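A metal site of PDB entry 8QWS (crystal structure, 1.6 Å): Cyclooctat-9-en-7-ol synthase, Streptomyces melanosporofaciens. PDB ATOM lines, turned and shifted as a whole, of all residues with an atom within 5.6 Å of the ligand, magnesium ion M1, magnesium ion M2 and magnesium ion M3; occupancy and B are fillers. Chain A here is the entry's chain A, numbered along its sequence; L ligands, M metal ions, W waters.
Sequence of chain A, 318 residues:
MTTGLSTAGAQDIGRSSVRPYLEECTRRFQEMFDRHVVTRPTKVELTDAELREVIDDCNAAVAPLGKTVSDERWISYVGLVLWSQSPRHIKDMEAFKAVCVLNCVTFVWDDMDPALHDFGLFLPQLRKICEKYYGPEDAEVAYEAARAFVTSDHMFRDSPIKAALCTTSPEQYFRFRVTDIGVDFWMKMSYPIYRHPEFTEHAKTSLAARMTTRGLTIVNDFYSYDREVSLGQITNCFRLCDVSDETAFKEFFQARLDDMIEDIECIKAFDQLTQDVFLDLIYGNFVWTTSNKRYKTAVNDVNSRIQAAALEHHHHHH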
ATOM      1  N   PHE A 107     -23.113  24.547  -0.435  1.00  0.00           N
ATOM      2  CA  PHE A 107     -22.953  24.398   1.020  1.00  0.00           C
ATOM      3  C   PHE A 107     -23.123  22.944   1.439  1.00  0.00           C
ATOM      4  O   PHE A 107     -22.388  22.454   2.318  1.00  0.00           O
ATOM      5  CB  PHE A 107     -23.974  25.271   1.755  1.00  0.00           C
ATOM      6  CG  PHE A 107     -23.414  26.559   2.255  1.00  0.00           C
ATOM      7  CD1 PHE A 107     -22.541  26.587   3.337  1.00  0.00           C
ATOM      8  CD2 PHE A 107     -23.759  27.744   1.645  1.00  0.00           C
ATOM      9  CE1 PHE A 107     -22.037  27.775   3.786  1.00  0.00           C
ATOM     10  CE2 PHE A 107     -23.241  28.950   2.086  1.00  0.00           C
ATOM     11  CZ  PHE A 107     -22.372  28.958   3.154  1.00  0.00           C
ATOM     12  N   ASP A 110     -20.024  21.136   0.350  1.00  0.00           N
ATOM     13  CA  ASP A 110     -18.907  21.531   1.212  1.00  0.00           C
ATOM     14  C   ASP A 110     -18.961  20.814   2.563  1.00  0.00           C
ATOM     15  O   ASP A 110     -17.925  20.566   3.164  1.00  0.00           O
ATOM     16  CB  ASP A 110     -18.953  23.055   1.418  1.00  0.00           C
ATOM     17  CG  ASP A 110     -17.791  23.587   2.274  1.00  0.00           C
ATOM     18  OD1 ASP A 110     -16.706  23.706   1.702  1.00  0.00           O
ATOM     19  OD2 ASP A 110     -17.992  23.940   3.498  1.00  0.00           O
ATOM     20  N   ASP A 111     -20.161  20.507   3.059  1.00  0.00           N
ATOM     21  CA  ASP A 111     -20.280  19.849   4.355  1.00  0.00           C
ATOM     22  C   ASP A 111     -20.229  18.327   4.290  1.00  0.00           C
ATOM     23  O   ASP A 111     -20.093  17.694   5.337  1.00  0.00           O
ATOM     24  CB  ASP A 111     -21.591  20.264   5.040  1.00  0.00           C
ATOM     25  CG  ASP A 111     -21.498  21.648   5.651  1.00  0.00           C
ATOM     26  OD1 ASP A 111     -20.375  22.171   5.802  1.00  0.00           O
ATOM     27  OD2 ASP A 111     -22.550  22.214   5.946  1.00  0.00           O
ATOM     28  N   PHE A 149     -15.633  24.289  -8.859  1.00  0.00           N
ATOM     29  CA  PHE A 149     -15.605  24.464  -7.417  1.00  0.00           C
ATOM     30  C   PHE A 149     -15.817  23.142  -6.693  1.00  0.00           C
ATOM     31  O   PHE A 149     -15.089  22.838  -5.733  1.00  0.00           O
ATOM     32  CB  PHE A 149     -16.672  25.465  -6.955  1.00  0.00           C
ATOM     33  CG  PHE A 149     -16.801  25.498  -5.449  1.00  0.00           C
ATOM     34  CD1 PHE A 149     -15.891  26.198  -4.669  1.00  0.00           C
ATOM     35  CD2 PHE A 149     -17.798  24.742  -4.821  1.00  0.00           C
ATOM     36  CE1 PHE A 149     -16.001  26.185  -3.282  1.00  0.00           C
ATOM     37  CE2 PHE A 149     -17.892  24.723  -3.445  1.00  0.00           C
ATOM     38  CZ  PHE A 149     -16.997  25.447  -2.682  1.00  0.00           C
ATOM     39  N   ASP A 153     -13.221  21.302  -4.252  1.00  0.00           N
ATOM     40  CA  ASP A 153     -13.480  20.935  -2.868  1.00  0.00           C
ATOM     41  C   ASP A 153     -13.181  19.459  -2.652  1.00  0.00           C
ATOM     42  O   ASP A 153     -12.588  19.073  -1.627  1.00  0.00           O
ATOM     43  CB  ASP A 153     -14.928  21.236  -2.505  1.00  0.00           C
ATOM     44  CG  ASP A 153     -15.277  20.708  -1.134  1.00  0.00           C
ATOM     45  OD1 ASP A 153     -14.708  21.233  -0.156  1.00  0.00           O
ATOM     46  OD2 ASP A 153     -16.093  19.766  -1.029  1.00  0.00           O
ATOM     47  N   ARG A 177      -7.676  30.245  -1.571  1.00  0.00           N
ATOM     48  CA  ARG A 177      -9.056  30.561  -1.247  1.00  0.00           C
ATOM     49  C   ARG A 177      -9.781  31.291  -2.371  1.00  0.00           C
ATOM     50  O   ARG A 177     -11.016  31.306  -2.350  1.00  0.00           O
ATOM     51  CB  ARG A 177      -9.099  31.363   0.059  1.00  0.00           C
ATOM     52  CG  ARG A 177      -8.758  30.422   1.221  1.00  0.00           C
ATOM     53  CD  ARG A 177      -9.917  29.411   1.447  1.00  0.00           C
ATOM     54  NE  ARG A 177     -10.611  29.709   2.706  1.00  0.00           N
ATOM     55  CZ  ARG A 177     -11.839  29.305   2.980  1.00  0.00           C
ATOM     56  NH1 ARG A 177     -12.527  28.541   2.136  1.00  0.00           N
ATOM     57  NH2 ARG A 177     -12.406  29.707   4.111  1.00  0.00           N
ATOM     58  N   ASP A 180     -11.253  28.220  -3.460  1.00  0.00           N
ATOM     59  CA  ASP A 180     -11.849  27.322  -2.464  1.00  0.00           C
ATOM     60  C   ASP A 180     -12.967  27.982  -1.631  1.00  0.00           C
ATOM     61  O   ASP A 180     -13.895  27.287  -1.159  1.00  0.00           O
ATOM     62  CB  ASP A 180     -10.772  26.792  -1.535  1.00  0.00           C
ATOM     63  CG  ASP A 180     -11.346  25.918  -0.441  1.00  0.00           C
ATOM     64  OD1 ASP A 180     -11.730  24.773  -0.728  1.00  0.00           O
ATOM     65  OD2 ASP A 180     -11.470  26.372   0.713  1.00  0.00           O
ATOM     66  N   ILE A 181     -12.890  29.289  -1.367  1.00  0.00           N
ATOM     67  CA  ILE A 181     -14.016  29.846  -0.609  1.00  0.00           C
ATOM     68  C   ILE A 181     -15.245  30.037  -1.475  1.00  0.00           C
ATOM     69  O   ILE A 181     -16.348  30.291  -0.957  1.00  0.00           O
ATOM     70  CB  ILE A 181     -13.631  31.171   0.063  1.00  0.00           C
ATOM     71  CG1 ILE A 181     -14.598  31.428   1.248  1.00  0.00           C
ATOM     72  CG2 ILE A 181     -13.628  32.319  -0.985  1.00  0.00           C
ATOM     73  CD1 ILE A 181     -14.114  32.374   2.215  1.00  0.00           C
ATOM     74  N   GLY A 182     -15.102  29.879  -2.798  1.00  0.00           N
ATOM     75  CA  GLY A 182     -16.262  29.901  -3.678  1.00  0.00           C
ATOM     76  C   GLY A 182     -16.507  31.229  -4.346  1.00  0.00           C
ATOM     77  O   GLY A 182     -17.514  31.388  -5.063  1.00  0.00           O
ATOM     78  N   ASN A 220     -15.021  35.025   7.133  1.00  0.00           N
ATOM     79  CA  ASN A 220     -15.489  33.654   7.335  1.00  0.00           C
ATOM     80  C   ASN A 220     -14.569  32.903   8.274  1.00  0.00           C
ATOM     81  O   ASN A 220     -15.031  32.123   9.126  1.00  0.00           O
ATOM     82  CB  ASN A 220     -15.601  32.907   6.012  1.00  0.00           C
ATOM     83  CG  ASN A 220     -15.966  31.452   6.264  1.00  0.00           C
ATOM     84  OD1 ASN A 220     -15.088  30.586   6.319  1.00  0.00           O
ATOM     85  ND2 ASN A 220     -17.253  31.206   6.535  1.00  0.00           N
ATOM     86  N   ASP A 221     -13.256  33.061   8.109  1.00  0.00           N
ATOM     87  CA  ASP A 221     -12.318  32.248   8.880  1.00  0.00           C
ATOM     88  C   ASP A 221     -12.457  32.545  10.362  1.00  0.00           C
ATOM     89  O   ASP A 221     -12.306  31.654  11.206  1.00  0.00           O
ATOM     90  CB  ASP A 221     -10.868  32.518   8.425  1.00  0.00           C
ATOM     91  CG  ASP A 221     -10.545  31.879   7.083  1.00  0.00           C
ATOM     92  OD1 ASP A 221     -11.351  31.103   6.581  1.00  0.00           O
ATOM     93  OD2 ASP A 221      -9.420  32.149   6.587  1.00  0.00           O
ATOM     94  N   SER A 224     -15.740  30.842  11.550  1.00  0.00           N
ATOM     95  CA  SER A 224     -15.842  29.402  11.377  1.00  0.00           C
ATOM     96  C   SER A 224     -14.653  28.653  11.965  1.00  0.00           C
ATOM     97  O   SER A 224     -14.634  27.404  11.934  1.00  0.00           O
ATOM     98  CB  SER A 224     -16.067  29.031   9.889  1.00  0.00           C
ATOM     99  OG  SER A 224     -14.976  29.438   9.076  1.00  0.00           O
ATOM    100  N   ARG A 227     -15.508  25.751  14.760  1.00  0.00           N
ATOM    101  CA  ARG A 227     -16.053  24.573  14.091  1.00  0.00           C
ATOM    102  C   ARG A 227     -14.977  23.847  13.306  1.00  0.00           C
ATOM    103  O   ARG A 227     -14.802  22.632  13.439  1.00  0.00           O
ATOM    104  CB  ARG A 227     -17.166  24.989  13.147  1.00  0.00           C
ATOM    105  CG  ARG A 227     -17.447  23.939  12.070  1.00  0.00           C
ATOM    106  CD  ARG A 227     -18.829  24.040  11.435  1.00  0.00           C
ATOM    107  NE  ARG A 227     -19.065  25.322  10.788  1.00  0.00           N
ATOM    108  CZ  ARG A 227     -18.581  25.703   9.610  1.00  0.00           C
ATOM    109  NH1 ARG A 227     -17.715  24.952   8.933  1.00  0.00           N
ATOM    110  NH2 ARG A 227     -18.937  26.878   9.103  1.00  0.00           N
ATOM    111  N   GLU A 228     -14.223  24.595  12.499  1.00  0.00           N
ATOM    112  CA  GLU A 228     -13.259  23.963  11.605  1.00  0.00           C
ATOM    113  C   GLU A 228     -12.172  23.232  12.389  1.00  0.00           C
ATOM    114  O   GLU A 228     -11.852  22.077  12.083  1.00  0.00           O
ATOM    115  CB  GLU A 228     -12.688  25.035  10.669  1.00  0.00           C
ATOM    116  CG  GLU A 228     -13.771  25.334   9.625  1.00  0.00           C
ATOM    117  CD  GLU A 228     -13.534  26.537   8.735  1.00  0.00           C
ATOM    118  OE1 GLU A 228     -12.433  27.132   8.774  1.00  0.00           O
ATOM    119  OE2 GLU A 228     -14.472  26.816   7.943  1.00  0.00           O
ATOM    120  N   GLN A 233     -10.251  20.506  10.185  1.00  0.00           N
ATOM    121  CA  GLN A 233     -10.083  21.208   8.921  1.00  0.00           C
ATOM    122  C   GLN A 233      -9.005  22.277   9.036  1.00  0.00           C
ATOM    123  O   GLN A 233      -8.945  22.999  10.025  1.00  0.00           O
ATOM    124  CB  GLN A 233     -11.419  21.813   8.490  1.00  0.00           C
ATOM    125  CG  GLN A 233     -12.464  20.773   8.066  1.00  0.00           C
ATOM    126  CD  GLN A 233     -13.877  21.318   7.912  1.00  0.00           C
ATOM    127  OE1 GLN A 233     -14.431  21.898   8.834  1.00  0.00           O
ATOM    128  NE2 GLN A 233     -14.479  21.121   6.745  1.00  0.00           N
ATOM    129  N   THR A 235      -8.237  24.679   6.583  1.00  0.00           N
ATOM    130  CA  THR A 235      -8.392  25.789   5.637  1.00  0.00           C
ATOM    131  C   THR A 235      -8.943  26.996   6.401  1.00  0.00           C
ATOM    132  O   THR A 235     -10.116  27.321   6.293  1.00  0.00           O
ATOM    133  CB  THR A 235      -9.303  25.374   4.492  1.00  0.00           C
ATOM    134  OG1 THR A 235      -8.780  24.179   3.889  1.00  0.00           O
ATOM    135  CG2 THR A 235      -9.271  26.429   3.403  1.00  0.00           C
ATOM    136  N   ASN A 236      -8.038  27.694   7.099  1.00  0.00           N
ATOM    137  CA  ASN A 236      -8.452  28.825   7.923  1.00  0.00           C
ATOM    138  C   ASN A 236      -7.216  29.630   8.270  1.00  0.00           C
ATOM    139  O   ASN A 236      -6.253  29.091   8.836  1.00  0.00           O
ATOM    140  CB  ASN A 236      -9.160  28.307   9.175  1.00  0.00           C
ATOM    141  CG  ASN A 236      -9.794  29.435   9.987  1.00  0.00           C
ATOM    142  OD1 ASN A 236      -9.122  30.395  10.375  1.00  0.00           O
ATOM    143  ND2 ASN A 236     -11.118  29.347  10.193  1.00  0.00           N
ATOM    144  N   TRP A 288     -24.431  38.587   7.276  1.00  0.00           N
ATOM    145  CA  TRP A 288     -25.032  37.261   7.287  1.00  0.00           C
ATOM    146  C   TRP A 288     -24.297  36.331   8.248  1.00  0.00           C
ATOM    147  O   TRP A 288     -24.940  35.569   8.983  1.00  0.00           O
ATOM    148  CB  TRP A 288     -25.057  36.666   5.882  1.00  0.00           C
ATOM    149  CG  TRP A 288     -25.420  35.209   5.814  1.00  0.00           C
ATOM    150  CD1 TRP A 288     -26.669  34.688   5.813  1.00  0.00           C
ATOM    151  CD2 TRP A 288     -24.518  34.092   5.696  1.00  0.00           C
ATOM    152  NE1 TRP A 288     -26.615  33.318   5.709  1.00  0.00           N
ATOM    153  CE2 TRP A 288     -25.302  32.922   5.667  1.00  0.00           C
ATOM    154  CE3 TRP A 288     -23.120  33.968   5.660  1.00  0.00           C
ATOM    155  CZ2 TRP A 288     -24.741  31.643   5.551  1.00  0.00           C
ATOM    156  CZ3 TRP A 288     -22.555  32.701   5.562  1.00  0.00           C
ATOM    157  CH2 TRP A 288     -23.374  31.549   5.508  1.00  0.00           C
ATOM    158  N   ARG A 294     -25.040  28.705  11.941  1.00  0.00           N
ATOM    159  CA  ARG A 294     -23.957  27.875  11.433  1.00  0.00           C
ATOM    160  C   ARG A 294     -22.647  28.185  12.138  1.00  0.00           C
ATOM    161  O   ARG A 294     -21.853  27.289  12.444  1.00  0.00           O
ATOM    162  CB  ARG A 294     -23.851  28.070   9.923  1.00  0.00           C
ATOM    163  CG  ARG A 294     -22.745  27.311   9.277  1.00  0.00           C
ATOM    164  CD  ARG A 294     -22.773  27.505   7.752  1.00  0.00           C
ATOM    165  NE  ARG A 294     -21.637  26.811   7.157  1.00  0.00           N
ATOM    166  CZ  ARG A 294     -21.649  25.536   6.805  1.00  0.00           C
ATOM    167  NH1 ARG A 294     -22.717  24.777   6.999  1.00  0.00           N
ATOM    168  NH2 ARG A 294     -20.568  25.012   6.225  1.00  0.00           N
ATOM    169  N   TYR A 295     -22.434  29.466  12.489  1.00  0.00           N
ATOM    170  CA  TYR A 295     -21.172  29.919  13.045  1.00  0.00           C
ATOM    171  C   TYR A 295     -21.233  30.187  14.551  1.00  0.00           C
ATOM    172  O   TYR A 295     -20.398  30.931  15.076  1.00  0.00           O
ATOM    173  CB  TYR A 295     -20.726  31.185  12.330  1.00  0.00           C
ATOM    174  CG  TYR A 295     -20.624  30.938  10.878  1.00  0.00           C
ATOM    175  CD1 TYR A 295     -19.689  29.999  10.390  1.00  0.00           C
ATOM    176  CD2 TYR A 295     -21.479  31.559   9.992  1.00  0.00           C
ATOM    177  CE1 TYR A 295     -19.612  29.732   9.044  1.00  0.00           C
ATOM    178  CE2 TYR A 295     -21.410  31.296   8.652  1.00  0.00           C
ATOM    179  CZ  TYR A 295     -20.453  30.391   8.181  1.00  0.00           C
ATOM    180  OH  TYR A 295     -20.405  30.111   6.854  1.00  0.00           O
HETATM  181  C1  LIG L   1     -18.273  27.475   1.789  1.00  0.00           C
HETATM  182  C2  LIG L   1     -18.626  28.896   1.346  1.00  0.00           C
HETATM  183  C3  LIG L   1     -18.366  27.228   3.290  1.00  0.00           C
HETATM  184  C4  LIG L   1     -17.390  27.982   4.199  1.00  0.00           C
HETATM  185  O1  LIG L   1     -19.247  27.883   6.212  1.00  0.00           O
HETATM  186  P1  LIG L   1     -17.802  27.499   5.947  1.00  0.00           P
HETATM  187  O2  LIG L   1     -16.957  28.147   6.960  1.00  0.00           O
HETATM  188  O3  LIG L   1     -17.655  26.001   6.016  1.00  0.00           O
HETATM  189  P2  LIG L   1     -15.657  27.451   3.863  1.00  0.00           P
HETATM  190  O4  LIG L   1     -15.670  25.945   3.711  1.00  0.00           O
HETATM  191  O5  LIG L   1     -14.772  27.803   4.982  1.00  0.00           O
HETATM  192  O6  LIG L   1     -15.183  28.149   2.614  1.00  0.00           O
HETATM  193  O7  LIG L   1     -17.401  29.379   4.088  1.00  0.00           O
HETATM  194  N1  LIG L   1     -17.471  29.765   1.591  1.00  0.00           N
HETATM  195 MG    MG M   1     -14.937  28.611   6.957  1.00  0.00          MG
HETATM  196 MG    MG M   2     -16.615  24.605   4.902  1.00  0.00          MG
HETATM  197 MG    MG M   3     -14.957  24.718   2.134  1.00  0.00          MG
HETATM  198  O   HOH W   1     -19.847  30.740   4.278  1.00  0.00           O
HETATM  199  O   HOH W   2     -12.882  28.991   7.166  1.00  0.00           O
HETATM  200  O   HOH W   3     -15.244  26.192   0.770  1.00  0.00           O
HETATM  201  O   HOH W   4     -14.923  23.424   3.721  1.00  0.00           O
HETATM  202  O   HOH W   5     -12.405  26.300   5.166  1.00  0.00           O
HETATM  203  O   HOH W   6     -12.969  25.353   2.563  1.00  0.00           O
HETATM  204  O   HOH W   7     -17.385  23.026   5.974  1.00  0.00           O
HETATM  205  O   HOH W   8     -13.992  23.527   0.565  1.00  0.00           O
HETATM  206  O   HOH W   9     -15.251  24.583   6.481  1.00  0.00           O
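The side-chain hydroxyl (OH) of Tyr 295 sits at hydrogen-bond distance from an oxygen (O1) of the ligand. The guanidinium group (NE) of Arg 294 is in salt-bridge range of an oxygen (O1) of the ligand, 2.8 Å away. The guanidinium group (NH2) of Arg 227 lies within salt-bridge range of an oxygen (O1) of the ligand (3.1 Å). N1 of the ligand lies within hydrogen-bond range of O of Ile 181 (2.8 Å). NH1 of Arg 177 is in salt-bridge range of O6 of the ligand.
The side-chain carboxylate (OD1) of Asp 221 is in salt-bridge range of the guanidinium group (NH2) of Arg 177. NH1 of Arg 294 lies within salt-bridge range of OD2 of Asp 111, at 2.8 Å. The side-chain amide nitrogen of Asn 236 lies within hydrogen-bond range of the side-chain carboxylate of Glu 228. ND2 of Asn 220 lies within hydrogen-bond range of OH of Tyr 295. The backbone carbonyl oxygen (O) of Glu 228 sits at hydrogen-bond distance from the backbone NH (N) of Gln 233 (2.9 Å). The guanidinium group (NH1) of Arg 177 is in salt-bridge range of the side-chain carboxylate (OD2) of Asp 180 (2.8 Å). The side-chain carboxylate (OE2) of Glu 228 lies close to the guanidinium group (NH1) of Arg 227, at 3.9 Å. OD2 of Asp 110 lies close to NH2 of Arg 294, at 3.9 Å.
Phe 107 touches the ligand (CE1 to O1, 3.7 Å). Hydrophobic or aromatic side chains that line the ligand: Phe 107, Ile 181 and Tyr 295. Within 4 Å of the ligand: Phe 107, Asp 110, Arg 177, Ile 181, Asn 220, Ser 224, Arg 227, Glu 228, Arg 294 and Tyr 295.
Arg 177 touches magnesium ion M1. Of the 20 residues printed, 4 come within 4 Å of magnesium ion M1. The nearest printed residue that does not touch magnesium ion M1 is Asp 221 (4.4 Å).
Within 4 Å of magnesium ion M2: Asp 110. The nearest printed residue that does not touch magnesium ion M2 is Arg 294 (4.2 Å).
Of the 20 residues printed, 1 comes within 4 Å of magnesium ion M3.
O2 of the ligand is bound to magnesium ion M1, at 2.1 Å. OD1 of Asn 220 binds magnesium ion M1 (2.1 Å). Magnesium ion M1 is bound by OE2 of Glu 228 (2.1 Å). Water W2 is bound to magnesium ion M1 (2.1 Å). An oxygen (O5) of the ligand binds magnesium ion M1 (2.1 Å). Magnesium ion M1 is bound by OG of Ser 224, at 2.3 Å.
Magnesium ion M2 is bound by O4 of the ligand (2.0 Å), water W7 (2.1 Å), O3 of the ligand (2.1 Å), OD2 of Asp 110 (2.1 Å), water W9 (2.1 Å) and water W4 (2.4 Å). Magnesium ion M2 has six donor atoms within binding distance.
Water W3 is bound to magnesium ion M3 (2.0 Å). Water W4 is bound to magnesium ion M3. OD1 of Asp 110 is bound to magnesium ion M3 (2.1 Å). O4 of the ligand is bound to magnesium ion M3. Magnesium ion M3 is bound by water W6 (2.1 Å). Water W8 is bound to magnesium ion M3 (2.2 Å). Magnesium ion M3 has six donor atoms within binding distance.
Water W6 lies within hydrogen-bond range of OD2 of Asp 180 (2.6 Å) and NH1 of Arg 177 (3.2 Å). Water W3 lies within hydrogen-bond range of the backbone carbonyl oxygen (O) of Asp 180 (2.6 Å) and an oxygen (O6) of the ligand (2.7 Å). Water W8 lies within hydrogen-bond range of OD1 of Asp 153 (2.5 Å) and OD1 of Asp 180 (2.9 Å). Water W1 lies within hydrogen-bond range of the side-chain hydroxyl (OH) of Tyr 295 (2.7 Å), an oxygen (O7) of the ligand (2.8 Å) and the side-chain amide nitrogen (ND2) of Asn 220 (3.5 Å).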
